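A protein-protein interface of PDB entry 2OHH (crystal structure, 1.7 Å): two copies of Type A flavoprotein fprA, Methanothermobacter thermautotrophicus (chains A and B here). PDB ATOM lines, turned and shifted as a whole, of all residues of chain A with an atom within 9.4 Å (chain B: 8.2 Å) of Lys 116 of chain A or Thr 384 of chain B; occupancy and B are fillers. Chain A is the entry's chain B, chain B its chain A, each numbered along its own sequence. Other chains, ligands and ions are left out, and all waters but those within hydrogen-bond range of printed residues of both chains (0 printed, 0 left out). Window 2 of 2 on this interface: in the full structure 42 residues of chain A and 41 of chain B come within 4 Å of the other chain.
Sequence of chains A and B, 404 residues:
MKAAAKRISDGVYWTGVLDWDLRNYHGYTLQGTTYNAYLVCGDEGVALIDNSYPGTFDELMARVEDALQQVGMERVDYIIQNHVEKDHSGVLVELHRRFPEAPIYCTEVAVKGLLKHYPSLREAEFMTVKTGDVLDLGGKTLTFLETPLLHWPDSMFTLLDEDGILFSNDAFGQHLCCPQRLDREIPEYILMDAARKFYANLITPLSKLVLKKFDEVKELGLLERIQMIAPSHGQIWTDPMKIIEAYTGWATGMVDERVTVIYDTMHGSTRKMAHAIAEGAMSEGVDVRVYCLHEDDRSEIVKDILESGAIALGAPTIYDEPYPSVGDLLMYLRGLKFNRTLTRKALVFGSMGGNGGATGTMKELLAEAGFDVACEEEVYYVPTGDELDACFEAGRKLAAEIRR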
ATOM      1  N   VAL A  84     -14.935  -5.729   5.475  1.00  0.00           N
ATOM      2  CA  VAL A  84     -15.501  -6.732   4.567  1.00  0.00           C
ATOM      3  C   VAL A  84     -15.544  -6.382   3.094  1.00  0.00           C
ATOM      4  O   VAL A  84     -15.810  -7.261   2.281  1.00  0.00           O
ATOM      5  CB  VAL A  84     -16.926  -7.189   4.982  1.00  0.00           C
ATOM      6  CG1 VAL A  84     -16.979  -7.522   6.449  1.00  0.00           C
ATOM      7  CG2 VAL A  84     -17.969  -6.151   4.640  1.00  0.00           C
ATOM      8  N   SER A  89     -11.326  -8.224   0.931  1.00  0.00           N
ATOM      9  CA  SER A  89     -11.815  -9.533   1.335  1.00  0.00           C
ATOM     10  C   SER A  89     -12.100 -10.429   0.137  1.00  0.00           C
ATOM     11  O   SER A  89     -12.625 -11.527   0.298  1.00  0.00           O
ATOM     12  CB  SER A  89     -13.082  -9.370   2.177  1.00  0.00           C
ATOM     13  OG  SER A  89     -14.154  -9.029   1.354  1.00  0.00           O
ATOM     14  N   LEU A  92     -10.641 -13.952   0.188  1.00  0.00           N
ATOM     15  CA  LEU A  92     -10.767 -14.568   1.500  1.00  0.00           C
ATOM     16  C   LEU A  92     -11.237 -16.014   1.357  1.00  0.00           C
ATOM     17  O   LEU A  92     -10.813 -16.888   2.116  1.00  0.00           O
ATOM     18  CB  LEU A  92     -11.771 -13.790   2.352  1.00  0.00           C
ATOM     19  CG  LEU A  92     -12.190 -14.423   3.687  1.00  0.00           C
ATOM     20  CD1 LEU A  92     -10.993 -14.570   4.596  1.00  0.00           C
ATOM     21  CD2 LEU A  92     -13.309 -13.633   4.373  1.00  0.00           C
ATOM     22  N   VAL A  93     -12.130 -16.245   0.399  1.00  0.00           N
ATOM     23  CA  VAL A  93     -12.612 -17.580   0.099  1.00  0.00           C
ATOM     24  C   VAL A  93     -11.429 -18.450  -0.325  1.00  0.00           C
ATOM     25  O   VAL A  93     -11.224 -19.546   0.228  1.00  0.00           O
ATOM     26  CB  VAL A  93     -13.755 -17.555  -0.939  1.00  0.00           C
ATOM     27  CG1 VAL A  93     -13.841 -18.866  -1.716  1.00  0.00           C
ATOM     28  CG2 VAL A  93     -15.063 -17.308  -0.229  1.00  0.00           C
ATOM     29  N   VAL A 109     -20.136  -7.592  13.335  1.00  0.00           N
ATOM     30  CA  VAL A 109     -20.834  -7.089  12.161  1.00  0.00           C
ATOM     31  C   VAL A 109     -20.175  -7.629  10.883  1.00  0.00           C
ATOM     32  O   VAL A 109     -20.868  -8.010   9.935  1.00  0.00           O
ATOM     33  CB  VAL A 109     -20.919  -5.541  12.170  1.00  0.00           C
ATOM     34  CG1 VAL A 109     -21.573  -5.021  10.895  1.00  0.00           C
ATOM     35  CG2 VAL A 109     -21.712  -5.069  13.390  1.00  0.00           C
ATOM     36  N   ALA A 110     -18.840  -7.688  10.876  1.00  0.00           N
ATOM     37  CA  ALA A 110     -18.125  -8.190   9.711  1.00  0.00           C
ATOM     38  C   ALA A 110     -18.462  -9.654   9.363  1.00  0.00           C
ATOM     39  O   ALA A 110     -18.468 -10.033   8.186  1.00  0.00           O
ATOM     40  CB  ALA A 110     -16.641  -7.995   9.858  1.00  0.00           C
ATOM     41  N   VAL A 111     -18.749 -10.477  10.368  1.00  0.00           N
ATOM     42  CA  VAL A 111     -19.158 -11.836  10.080  1.00  0.00           C
ATOM     43  C   VAL A 111     -20.392 -11.850   9.190  1.00  0.00           C
ATOM     44  O   VAL A 111     -20.403 -12.535   8.172  1.00  0.00           O
ATOM     45  CB  VAL A 111     -19.405 -12.661  11.332  1.00  0.00           C
ATOM     46  CG1 VAL A 111     -19.730 -14.101  10.934  1.00  0.00           C
ATOM     47  CG2 VAL A 111     -18.190 -12.630  12.208  1.00  0.00           C
ATOM     48  N   LYS A 112     -21.413 -11.072   9.552  1.00  0.00           N
ATOM     49  CA  LYS A 112     -22.650 -10.999   8.754  1.00  0.00           C
ATOM     50  C   LYS A 112     -22.356 -10.519   7.333  1.00  0.00           C
ATOM     51  O   LYS A 112     -22.878 -11.067   6.367  1.00  0.00           O
ATOM     52  CB  LYS A 112     -23.712 -10.092   9.415  1.00  0.00           C
ATOM     53  CG  LYS A 112     -24.099 -10.521  10.839  1.00  0.00           C
ATOM     54  CD  LYS A 112     -24.501 -12.041  10.922  1.00  0.00           C
ATOM     55  CE  LYS A 112     -23.980 -12.725  12.200  1.00  0.00           C
ATOM     56  NZ  LYS A 112     -22.581 -12.275  12.554  1.00  0.00           N
ATOM     57  N   GLY A 113     -21.497  -9.508   7.234  1.00  0.00           N
ATOM     58  CA  GLY A 113     -21.108  -8.917   5.959  1.00  0.00           C
ATOM     59  C   GLY A 113     -20.329  -9.908   5.129  1.00  0.00           C
ATOM     60  O   GLY A 113     -20.600 -10.094   3.954  1.00  0.00           O
ATOM     61  N   LEU A 114     -19.363 -10.571   5.753  1.00  0.00           N
ATOM     62  CA  LEU A 114     -18.554 -11.554   5.041  1.00  0.00           C
ATOM     63  C   LEU A 114     -19.416 -12.709   4.543  1.00  0.00           C
ATOM     64  O   LEU A 114     -19.294 -13.131   3.386  1.00  0.00           O
ATOM     65  CB  LEU A 114     -17.397 -12.052   5.925  1.00  0.00           C
ATOM     66  CG  LEU A 114     -16.315 -11.001   6.180  1.00  0.00           C
ATOM     67  CD1 LEU A 114     -15.282 -11.475   7.179  1.00  0.00           C
ATOM     68  CD2 LEU A 114     -15.661 -10.611   4.878  1.00  0.00           C
ATOM     69  N   LEU A 115     -20.318 -13.183   5.402  1.00  0.00           N
ATOM     70  CA  LEU A 115     -21.177 -14.314   5.074  1.00  0.00           C
ATOM     71  C   LEU A 115     -22.116 -13.987   3.935  1.00  0.00           C
ATOM     72  O   LEU A 115     -22.476 -14.853   3.136  1.00  0.00           O
ATOM     73  CB  LEU A 115     -21.963 -14.780   6.309  1.00  0.00           C
ATOM     74  CG  LEU A 115     -21.251 -15.660   7.337  1.00  0.00           C
ATOM     75  CD1 LEU A 115     -22.157 -15.828   8.555  1.00  0.00           C
ATOM     76  CD2 LEU A 115     -21.013 -17.014   6.731  1.00  0.00           C
ATOM     77  N   LYS A 116     -22.531 -12.734   3.861  1.00  0.00           N
ATOM     78  CA  LYS A 116     -23.354 -12.322   2.747  1.00  0.00           C
ATOM     79  C   LYS A 116     -22.592 -12.302   1.414  1.00  0.00           C
ATOM     80  O   LYS A 116     -23.129 -12.704   0.375  1.00  0.00           O
ATOM     81  CB  LYS A 116     -23.949 -10.948   2.993  1.00  0.00           C
ATOM     82  CG  LYS A 116     -25.141 -10.715   2.113  1.00  0.00           C
ATOM     83  CD  LYS A 116     -26.315 -11.536   2.661  1.00  0.00           C
ATOM     84  CE  LYS A 116     -27.228 -12.040   1.560  1.00  0.00           C
ATOM     85  NZ  LYS A 116     -27.902 -10.947   0.844  1.00  0.00           N
ATOM     86  N   HIS A 117     -21.359 -11.819   1.438  1.00  0.00           N
ATOM     87  CA  HIS A 117     -20.556 -11.819   0.227  1.00  0.00           C
ATOM     88  C   HIS A 117     -20.152 -13.203  -0.209  1.00  0.00           C
ATOM     89  O   HIS A 117     -20.133 -13.503  -1.399  1.00  0.00           O
ATOM     90  CB  HIS A 117     -19.295 -10.999   0.420  1.00  0.00           C
ATOM     91  CG  HIS A 117     -19.534  -9.527   0.421  1.00  0.00           C
ATOM     92  ND1 HIS A 117     -19.988  -8.856   1.533  1.00  0.00           N
ATOM     93  CD2 HIS A 117     -19.378  -8.599  -0.552  1.00  0.00           C
ATOM     94  CE1 HIS A 117     -20.077  -7.569   1.250  1.00  0.00           C
ATOM     95  NE2 HIS A 117     -19.721  -7.386  -0.009  1.00  0.00           N
ATOM     96  N   TYR A 118     -19.809 -14.034   0.763  1.00  0.00           N
ATOM     97  CA  TYR A 118     -19.246 -15.334   0.476  1.00  0.00           C
ATOM     98  C   TYR A 118     -19.988 -16.373   1.314  1.00  0.00           C
ATOM     99  O   TYR A 118     -19.555 -16.725   2.412  1.00  0.00           O
ATOM    100  CB  TYR A 118     -17.740 -15.321   0.762  1.00  0.00           C
ATOM    101  CG  TYR A 118     -17.089 -14.012   0.353  1.00  0.00           C
ATOM    102  CD1 TYR A 118     -17.074 -13.619  -0.980  1.00  0.00           C
ATOM    103  CD2 TYR A 118     -16.505 -13.165   1.301  1.00  0.00           C
ATOM    104  CE1 TYR A 118     -16.498 -12.404  -1.369  1.00  0.00           C
ATOM    105  CE2 TYR A 118     -15.916 -11.947   0.924  1.00  0.00           C
ATOM    106  CZ  TYR A 118     -15.927 -11.585  -0.416  1.00  0.00           C
ATOM    107  OH  TYR A 118     -15.368 -10.414  -0.836  1.00  0.00           O
ATOM    108  N   PRO A 119     -21.136 -16.831   0.813  1.00  0.00           N
ATOM    109  CA  PRO A 119     -21.973 -17.789   1.562  1.00  0.00           C
ATOM    110  C   PRO A 119     -21.226 -19.062   1.949  1.00  0.00           C
ATOM    111  O   PRO A 119     -21.504 -19.641   3.004  1.00  0.00           O
ATOM    112  CB  PRO A 119     -23.096 -18.120   0.574  1.00  0.00           C
ATOM    113  CG  PRO A 119     -23.122 -16.977  -0.359  1.00  0.00           C
ATOM    114  CD  PRO A 119     -21.740 -16.469  -0.484  1.00  0.00           C
ATOM    115  N   SER A 120     -20.276 -19.471   1.104  1.00  0.00           N
ATOM    116  CA  SER A 120     -19.470 -20.665   1.328  1.00  0.00           C
ATOM    117  C   SER A 120     -18.661 -20.635   2.647  1.00  0.00           C
ATOM    118  O   SER A 120     -18.133 -21.660   3.101  1.00  0.00           O
ATOM    119  CB  SER A 120     -18.554 -20.900   0.120  1.00  0.00           C
ATOM    120  OG  SER A 120     -17.498 -19.950   0.053  1.00  0.00           O
ATOM    121  N   LEU A 121     -18.576 -19.459   3.262  1.00  0.00           N
ATOM    122  CA  LEU A 121     -17.875 -19.283   4.532  1.00  0.00           C
ATOM    123  C   LEU A 121     -18.737 -19.610   5.748  1.00  0.00           C
ATOM    124  O   LEU A 121     -18.294 -19.463   6.889  1.00  0.00           O
ATOM    125  CB  LEU A 121     -17.318 -17.863   4.638  1.00  0.00           C
ATOM    126  CG  LEU A 121     -16.192 -17.555   3.656  1.00  0.00           C
ATOM    127  CD1 LEU A 121     -15.851 -16.089   3.730  1.00  0.00           C
ATOM    128  CD2 LEU A 121     -14.962 -18.387   3.947  1.00  0.00           C
ATOM    129  N   ARG A 122     -19.968 -20.048   5.500  1.00  0.00           N
ATOM    130  CA  ARG A 122     -20.834 -20.631   6.534  1.00  0.00           C
ATOM    131  C   ARG A 122     -20.106 -21.689   7.361  1.00  0.00           C
ATOM    132  O   ARG A 122     -20.332 -21.822   8.559  1.00  0.00           O
ATOM    133  CB  ARG A 122     -22.075 -21.244   5.884  1.00  0.00           C
ATOM    134  CG  ARG A 122     -21.790 -22.411   4.914  1.00  0.00           C
ATOM    135  CD  ARG A 122     -23.000 -22.721   4.035  1.00  0.00           C
ATOM    136  NE  ARG A 122     -24.211 -22.853   4.840  1.00  0.00           N
ATOM    137  CZ  ARG A 122     -25.307 -22.101   4.704  1.00  0.00           C
ATOM    138  NH1 ARG A 122     -25.369 -21.146   3.769  1.00  0.00           N
ATOM    139  NH2 ARG A 122     -26.354 -22.310   5.499  1.00  0.00           N
ATOM    140  N   PHE A 126     -15.028 -18.491  12.479  1.00  0.00           N
ATOM    141  CA  PHE A 126     -14.832 -17.080  12.757  1.00  0.00           C
ATOM    142  C   PHE A 126     -14.557 -16.836  14.230  1.00  0.00           C
ATOM    143  O   PHE A 126     -15.272 -17.325  15.108  1.00  0.00           O
ATOM    144  CB  PHE A 126     -16.050 -16.249  12.344  1.00  0.00           C
ATOM    145  CG  PHE A 126     -16.265 -16.156  10.867  1.00  0.00           C
ATOM    146  CD1 PHE A 126     -15.711 -15.107  10.138  1.00  0.00           C
ATOM    147  CD2 PHE A 126     -17.068 -17.084  10.207  1.00  0.00           C
ATOM    148  CE1 PHE A 126     -15.929 -14.999   8.771  1.00  0.00           C
ATOM    149  CE2 PHE A 126     -17.288 -16.980   8.838  1.00  0.00           C
ATOM    150  CZ  PHE A 126     -16.713 -15.936   8.123  1.00  0.00           C
ATOM    151  N   SER B 269     -23.492  -5.729  -7.246  1.00  0.00           N
ATOM    152  CA  SER B 269     -24.683  -6.370  -6.712  1.00  0.00           C
ATOM    153  C   SER B 269     -25.921  -5.749  -7.279  1.00  0.00           C
ATOM    154  O   SER B 269     -26.868  -6.438  -7.638  1.00  0.00           O
ATOM    155  CB  SER B 269     -24.700  -6.277  -5.204  1.00  0.00           C
ATOM    156  OG  SER B 269     -23.669  -7.117  -4.721  1.00  0.00           O
ATOM    157  N   LYS B 272     -26.415  -7.175 -10.623  1.00  0.00           N
ATOM    158  CA  LYS B 272     -27.050  -8.494 -10.594  1.00  0.00           C
ATOM    159  C   LYS B 272     -28.562  -8.334 -10.410  1.00  0.00           C
ATOM    160  O   LYS B 272     -29.372  -8.988 -11.092  1.00  0.00           O
ATOM    161  CB  LYS B 272     -26.469  -9.320  -9.452  1.00  0.00           C
ATOM    162  CG  LYS B 272     -25.095  -9.881  -9.753  1.00  0.00           C
ATOM    163  CD  LYS B 272     -24.437 -10.430  -8.470  1.00  0.00           C
ATOM    164  CE  LYS B 272     -23.033 -10.914  -8.783  1.00  0.00           C
ATOM    165  NZ  LYS B 272     -22.655 -10.427 -10.163  1.00  0.00           N
ATOM    166  N   MET B 273     -28.950  -7.455  -9.487  1.00  0.00           N
ATOM    167  CA  MET B 273     -30.368  -7.204  -9.283  1.00  0.00           C
ATOM    168  C   MET B 273     -31.035  -6.714 -10.550  1.00  0.00           C
ATOM    169  O   MET B 273     -32.100  -7.168 -10.912  1.00  0.00           O
ATOM    170  CB  MET B 273     -30.584  -6.191  -8.181  1.00  0.00           C
ATOM    171  CG  MET B 273     -30.034  -6.672  -6.861  1.00  0.00           C
ATOM    172  SD  MET B 273     -30.079  -5.446  -5.567  1.00  0.00           S
ATOM    173  CE  MET B 273     -31.796  -5.317  -5.184  1.00  0.00           C
ATOM    174  N   ALA B 276     -31.759  -9.404 -13.005  1.00  0.00           N
ATOM    175  CA  ALA B 276     -32.840 -10.271 -12.574  1.00  0.00           C
ATOM    176  C   ALA B 276     -34.161  -9.602 -12.796  1.00  0.00           C
ATOM    177  O   ALA B 276     -35.088 -10.224 -13.264  1.00  0.00           O
ATOM    178  CB  ALA B 276     -32.695 -10.668 -11.085  1.00  0.00           C
ATOM    179  N   SER B 351     -28.427  -2.522  -3.708  1.00  0.00           N
ATOM    180  CA  SER B 351     -27.764  -3.232  -2.659  1.00  0.00           C
ATOM    181  C   SER B 351     -27.296  -2.219  -1.624  1.00  0.00           C
ATOM    182  O   SER B 351     -27.104  -1.030  -1.912  1.00  0.00           O
ATOM    183  CB  SER B 351     -26.579  -3.986  -3.239  1.00  0.00           C
ATOM    184  OG  SER B 351     -25.995  -4.740  -2.210  1.00  0.00           O
ATOM    185  N   MET B 352     -27.098  -2.669  -0.401  1.00  0.00           N
ATOM    186  CA  MET B 352     -26.520  -1.749   0.552  1.00  0.00           C
ATOM    187  C   MET B 352     -25.783  -2.572   1.578  1.00  0.00           C
ATOM    188  O   MET B 352     -25.835  -3.809   1.522  1.00  0.00           O
ATOM    189  CB  MET B 352     -27.613  -0.881   1.161  1.00  0.00           C
ATOM    190  CG  MET B 352     -28.841  -1.649   1.569  1.00  0.00           C
ATOM    191  SD  MET B 352     -28.586  -2.382   3.180  1.00  0.00           S
ATOM    192  CE  MET B 352     -30.083  -3.359   3.323  1.00  0.00           C
ATOM    193  N   GLU B 378     -34.647  -4.206  -1.851  1.00  0.00           N
ATOM    194  CA  GLU B 378     -33.355  -3.810  -1.271  1.00  0.00           C
ATOM    195  C   GLU B 378     -32.632  -5.044  -0.749  1.00  0.00           C
ATOM    196  O   GLU B 378     -33.259  -5.885  -0.111  1.00  0.00           O
ATOM    197  CB  GLU B 378     -33.573  -2.741  -0.184  1.00  0.00           C
ATOM    198  CG  GLU B 378     -32.312  -2.332   0.605  1.00  0.00           C
ATOM    199  CD  GLU B 378     -32.562  -1.183   1.588  1.00  0.00           C
ATOM    200  OE1 GLU B 378     -33.162  -1.434   2.666  1.00  0.00           O
ATOM    201  OE2 GLU B 378     -32.148  -0.031   1.306  1.00  0.00           O
ATOM    202  N   VAL B 379     -31.336  -5.162  -1.053  1.00  0.00           N
ATOM    203  CA  VAL B 379     -30.569  -6.362  -0.761  1.00  0.00           C
ATOM    204  C   VAL B 379     -29.359  -5.954   0.039  1.00  0.00           C
ATOM    205  O   VAL B 379     -28.804  -4.892  -0.172  1.00  0.00           O
ATOM    206  CB  VAL B 379     -30.225  -7.143  -2.060  1.00  0.00           C
ATOM    207  CG1 VAL B 379     -29.121  -8.112  -1.854  1.00  0.00           C
ATOM    208  CG2 VAL B 379     -31.484  -7.912  -2.516  1.00  0.00           C
ATOM    209  N   TYR B 380     -29.013  -6.761   1.025  1.00  0.00           N
ATOM    210  CA  TYR B 380     -27.834  -6.496   1.798  1.00  0.00           C
ATOM    211  C   TYR B 380     -26.687  -7.117   1.030  1.00  0.00           C
ATOM    212  O   TYR B 380     -26.655  -8.330   0.828  1.00  0.00           O
ATOM    213  CB  TYR B 380     -28.029  -7.179   3.132  1.00  0.00           C
ATOM    214  CG  TYR B 380     -26.878  -7.123   4.070  1.00  0.00           C
ATOM    215  CD1 TYR B 380     -26.338  -5.900   4.484  1.00  0.00           C
ATOM    216  CD2 TYR B 380     -26.362  -8.288   4.578  1.00  0.00           C
ATOM    217  CE1 TYR B 380     -25.293  -5.860   5.390  1.00  0.00           C
ATOM    218  CE2 TYR B 380     -25.315  -8.263   5.468  1.00  0.00           C
ATOM    219  CZ  TYR B 380     -24.798  -7.053   5.876  1.00  0.00           C
ATOM    220  OH  TYR B 380     -23.763  -7.055   6.768  1.00  0.00           O
ATOM    221  N   TYR B 381     -25.771  -6.279   0.563  1.00  0.00           N
ATOM    222  CA  TYR B 381     -24.605  -6.742  -0.179  1.00  0.00           C
ATOM    223  C   TYR B 381     -25.018  -7.600  -1.380  1.00  0.00           C
ATOM    224  O   TYR B 381     -25.814  -7.157  -2.215  1.00  0.00           O
ATOM    225  CB  TYR B 381     -23.632  -7.451   0.743  1.00  0.00           C
ATOM    226  CG  TYR B 381     -22.930  -6.514   1.688  1.00  0.00           C
ATOM    227  CD1 TYR B 381     -22.284  -5.387   1.214  1.00  0.00           C
ATOM    228  CD2 TYR B 381     -22.906  -6.750   3.050  1.00  0.00           C
ATOM    229  CE1 TYR B 381     -21.600  -4.534   2.078  1.00  0.00           C
ATOM    230  CE2 TYR B 381     -22.241  -5.898   3.916  1.00  0.00           C
ATOM    231  CZ  TYR B 381     -21.602  -4.785   3.425  1.00  0.00           C
ATOM    232  OH  TYR B 381     -20.936  -3.944   4.286  1.00  0.00           O
ATOM    233  N   VAL B 382     -24.492  -8.818  -1.446  1.00  0.00           N
ATOM    234  CA  VAL B 382     -24.631  -9.644  -2.628  1.00  0.00           C
ATOM    235  C   VAL B 382     -25.927 -10.400  -2.551  1.00  0.00           C
ATOM    236  O   VAL B 382     -26.166 -11.071  -1.570  1.00  0.00           O
ATOM    237  CB  VAL B 382     -23.492 -10.657  -2.768  1.00  0.00           C
ATOM    238  CG1 VAL B 382     -23.734 -11.522  -3.996  1.00  0.00           C
ATOM    239  CG2 VAL B 382     -22.135  -9.919  -2.880  1.00  0.00           C
ATOM    240  N   PRO B 383     -26.774 -10.261  -3.579  1.00  0.00           N
ATOM    241  CA  PRO B 383     -28.058 -10.970  -3.608  1.00  0.00           C
ATOM    242  C   PRO B 383     -27.904 -12.484  -3.585  1.00  0.00           C
ATOM    243  O   PRO B 383     -27.084 -13.063  -4.322  1.00  0.00           O
ATOM    244  CB  PRO B 383     -28.708 -10.509  -4.922  1.00  0.00           C
ATOM    245  CG  PRO B 383     -27.687  -9.773  -5.656  1.00  0.00           C
ATOM    246  CD  PRO B 383     -26.608  -9.365  -4.740  1.00  0.00           C
ATOM    247  N   THR B 384     -28.679 -13.118  -2.725  1.00  0.00           N
ATOM    248  CA  THR B 384     -28.723 -14.559  -2.731  1.00  0.00           C
ATOM    249  C   THR B 384     -29.547 -14.979  -3.959  1.00  0.00           C
ATOM    250  O   THR B 384     -30.135 -14.134  -4.617  1.00  0.00           O
ATOM    251  CB  THR B 384     -29.412 -15.074  -1.472  1.00  0.00           C
ATOM    252  OG1 THR B 384     -30.735 -14.550  -1.451  1.00  0.00           O
ATOM    253  CG2 THR B 384     -28.648 -14.612  -0.224  1.00  0.00           C
ATOM    254  N   GLY B 385     -29.543 -16.272  -4.280  1.00  0.00           N
ATOM    255  CA  GLY B 385     -30.448 -16.831  -5.280  1.00  0.00           C
ATOM    256  C   GLY B 385     -31.907 -16.467  -5.013  1.00  0.00           C
ATOM    257  O   GLY B 385     -32.602 -16.046  -5.930  1.00  0.00           O
ATOM    258  N   ASP B 386     -32.364 -16.624  -3.766  1.00  0.00           N
ATOM    259  CA  ASP B 386     -33.712 -16.192  -3.358  1.00  0.00           C
ATOM    260  C   ASP B 386     -33.972 -14.723  -3.621  1.00  0.00           C
ATOM    261  O   ASP B 386     -35.047 -14.342  -4.064  1.00  0.00           O
ATOM    262  CB  ASP B 386     -33.942 -16.433  -1.864  1.00  0.00           C
ATOM    263  CG  ASP B 386     -34.436 -17.851  -1.562  1.00  0.00           C
ATOM    264  OD1 ASP B 386     -34.496 -18.679  -2.509  1.00  0.00           O
ATOM    265  OD2 ASP B 386     -34.770 -18.131  -0.378  1.00  0.00           O
ATOM    266  N   GLU B 387     -32.988 -13.893  -3.304  1.00  0.00           N
ATOM    267  CA  GLU B 387     -33.131 -12.452  -3.493  1.00  0.00           C
ATOM    268  C   GLU B 387     -33.172 -12.094  -4.974  1.00  0.00           C
ATOM    269  O   GLU B 387     -33.892 -11.229  -5.377  1.00  0.00           O
ATOM    270  CB  GLU B 387     -32.050 -11.690  -2.719  1.00  0.00           C
ATOM    271  CG  GLU B 387     -32.278 -11.784  -1.203  1.00  0.00           C
ATOM    272  CD  GLU B 387     -31.080 -11.366  -0.366  1.00  0.00           C
ATOM    273  OE1 GLU B 387     -29.905 -11.459  -0.837  1.00  0.00           O
ATOM    274  OE2 GLU B 387     -31.335 -10.934   0.784  1.00  0.00           O
ATOM    275  N   LEU B 388     -32.405 -12.803  -5.779  1.00  0.00           N
ATOM    276  CA  LEU B 388     -32.359 -12.560  -7.200  1.00  0.00           C
ATOM    277  C   LEU B 388     -33.657 -13.056  -7.768  1.00  0.00           C
ATOM    278  O   LEU B 388     -34.209 -12.423  -8.638  1.00  0.00           O
ATOM    279  CB  LEU B 388     -31.168 -13.290  -7.814  1.00  0.00           C
ATOM    280  CG  LEU B 388     -30.215 -12.446  -8.699  1.00  0.00           C
ATOM    281  CD1 LEU B 388     -29.962 -11.011  -8.196  1.00  0.00           C
ATOM    282  CD2 LEU B 388     -28.908 -13.200  -8.880  1.00  0.00           C
ATOM    283  N   ASP B 389     -34.182 -14.156  -7.232  1.00  0.00           N
ATOM    284  CA  ASP B 389     -35.526 -14.613  -7.609  1.00  0.00           C
ATOM    285  C   ASP B 389     -36.566 -13.571  -7.290  1.00  0.00           C
ATOM    286  O   ASP B 389     -37.460 -13.341  -8.084  1.00  0.00           O
ATOM    287  CB  ASP B 389     -35.892 -15.930  -6.939  1.00  0.00           C
ATOM    288  CG  ASP B 389     -35.219 -17.117  -7.605  1.00  0.00           C
ATOM    289  OD1 ASP B 389     -34.523 -16.902  -8.626  1.00  0.00           O
ATOM    290  OD2 ASP B 389     -35.367 -18.251  -7.104  1.00  0.00           O
ATOM    291  N   ALA B 390     -36.428 -12.930  -6.131  1.00  0.00           N
ATOM    292  CA  ALA B 390     -37.350 -11.862  -5.724  1.00  0.00           C
ATOM    293  C   ALA B 390     -37.194 -10.652  -6.641  1.00  0.00           C
ATOM    294  O   ALA B 390     -38.162  -9.960  -6.932  1.00  0.00           O
ATOM    295  CB  ALA B 390     -37.092 -11.473  -4.290  1.00  0.00           C
ATOM    296  N   CYS B 391     -35.973 -10.394  -7.110  1.00  0.00           N
ATOM    297  CA  CYS B 391     -35.811  -9.310  -8.101  1.00  0.00           C
ATOM    298  C   CYS B 391     -36.503  -9.654  -9.427  1.00  0.00           C
ATOM    299  O   CYS B 391     -37.079  -8.782 -10.088  1.00  0.00           O
ATOM    300  CB  CYS B 391     -34.325  -9.026  -8.381  1.00  0.00           C
ATOM    301  SG  CYS B 391     -33.460  -8.264  -6.999  1.00  0.00           S
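Of the 19 printed residues of chain A, 5 touch a printed residue of chain B. Printed residues of chain A that touch a printed residue of chain B: Val 84, Lys 112, Gly 113, Lys 116 and His 117. Hydrophobic or aromatic side chains of chain A within 4 Å of the printed part of chain B: Val 84 and His 117. Printed residues of chain B that touch a printed residue of chain A: Tyr 380, Tyr 381, Val 382, Thr 384 and Glu 387. Among the printed residues, 11 pairs touch across the chains.
Printed residues of chain A within 4 Å of Val 382 of chain B: Lys 116 (3.0 Å) and His 117 (3.8 Å). No residue of chain A comes within 4 Å of Pro 383 of chain B. Gly 385 of chain B touches none of the printed residues of chain A. Glu 387 of chain B touches just one residue of chain A: Lys 116. Of the printed residues of chain B, Val 84 of chain A touches Tyr 381 (3.7 Å). Printed residues of chain B within 4 Å of Gly 113 of chain A: Tyr 380 and Tyr 381. Lys 272 of chain B touches none of the printed residues of chain A. Val 93 of chain A touches none of the printed residues of chain B. The nearest residue of chain B that does not touch Lys 116 of chain A is Val 379 of chain B (4.1 Å). The nearest printed residue of chain B that does not touch His 117 of chain A is Ser 269 of chain B (6.2 Å).
The backbone carbonyl oxygen (O) of Val 382 of chain B is in hydrogen-bond range of the side-chain amino group (NZ) of Lys 116 of chain A (3.0 Å). The side-chain carboxylate (OE1) of Glu 387 of chain B is in salt-bridge range of the side-chain amino group (NZ) of Lys 116 of chain A, at 2.7 Å. O of Tyr 380 of chain B is in hydrogen-bond range of NZ of Lys 116 of chain A (2.9 Å). The side-chain hydroxyl (OH) of Tyr 380 of chain B lies close to the backbone NH (N) of Gly 113 of chain A.
Among the printed residues, merely in contact across the chains: Val 84 of chain A with Tyr 381 of chain B, Lys 112 of chain A with Tyr 380 of chain B, Gly 113 of chain A with Tyr 381 of chain B, Lys 116 of chain A with Tyr 381 of chain B, Lys 116 of chain A with Thr 384 of chain B, His 117 of chain A with Tyr 381 of chain B and His 117 of chain A with Val 382 of chain B.
No position is printed for both chains.
The backbone NH (N) of Thr 384 of chain B sits at hydrogen-bond distance from the side-chain carboxylate (OE1) of Glu 387 of chain B, 2.8 Å away. O of Tyr 381 of chain B sits at hydrogen-bond distance from OG of Ser 351 of chain B (2.4 Å). The backbone carbonyl oxygen of Met 352 of chain B sits at hydrogen-bond distance from the backbone NH of Tyr 381 of chain B, at 2.7 Å. A ring nitrogen (ND1) of His 117 of chain A is in hydrogen-bond range of the backbone carbonyl oxygen (O) of Gly 113 of chain A.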
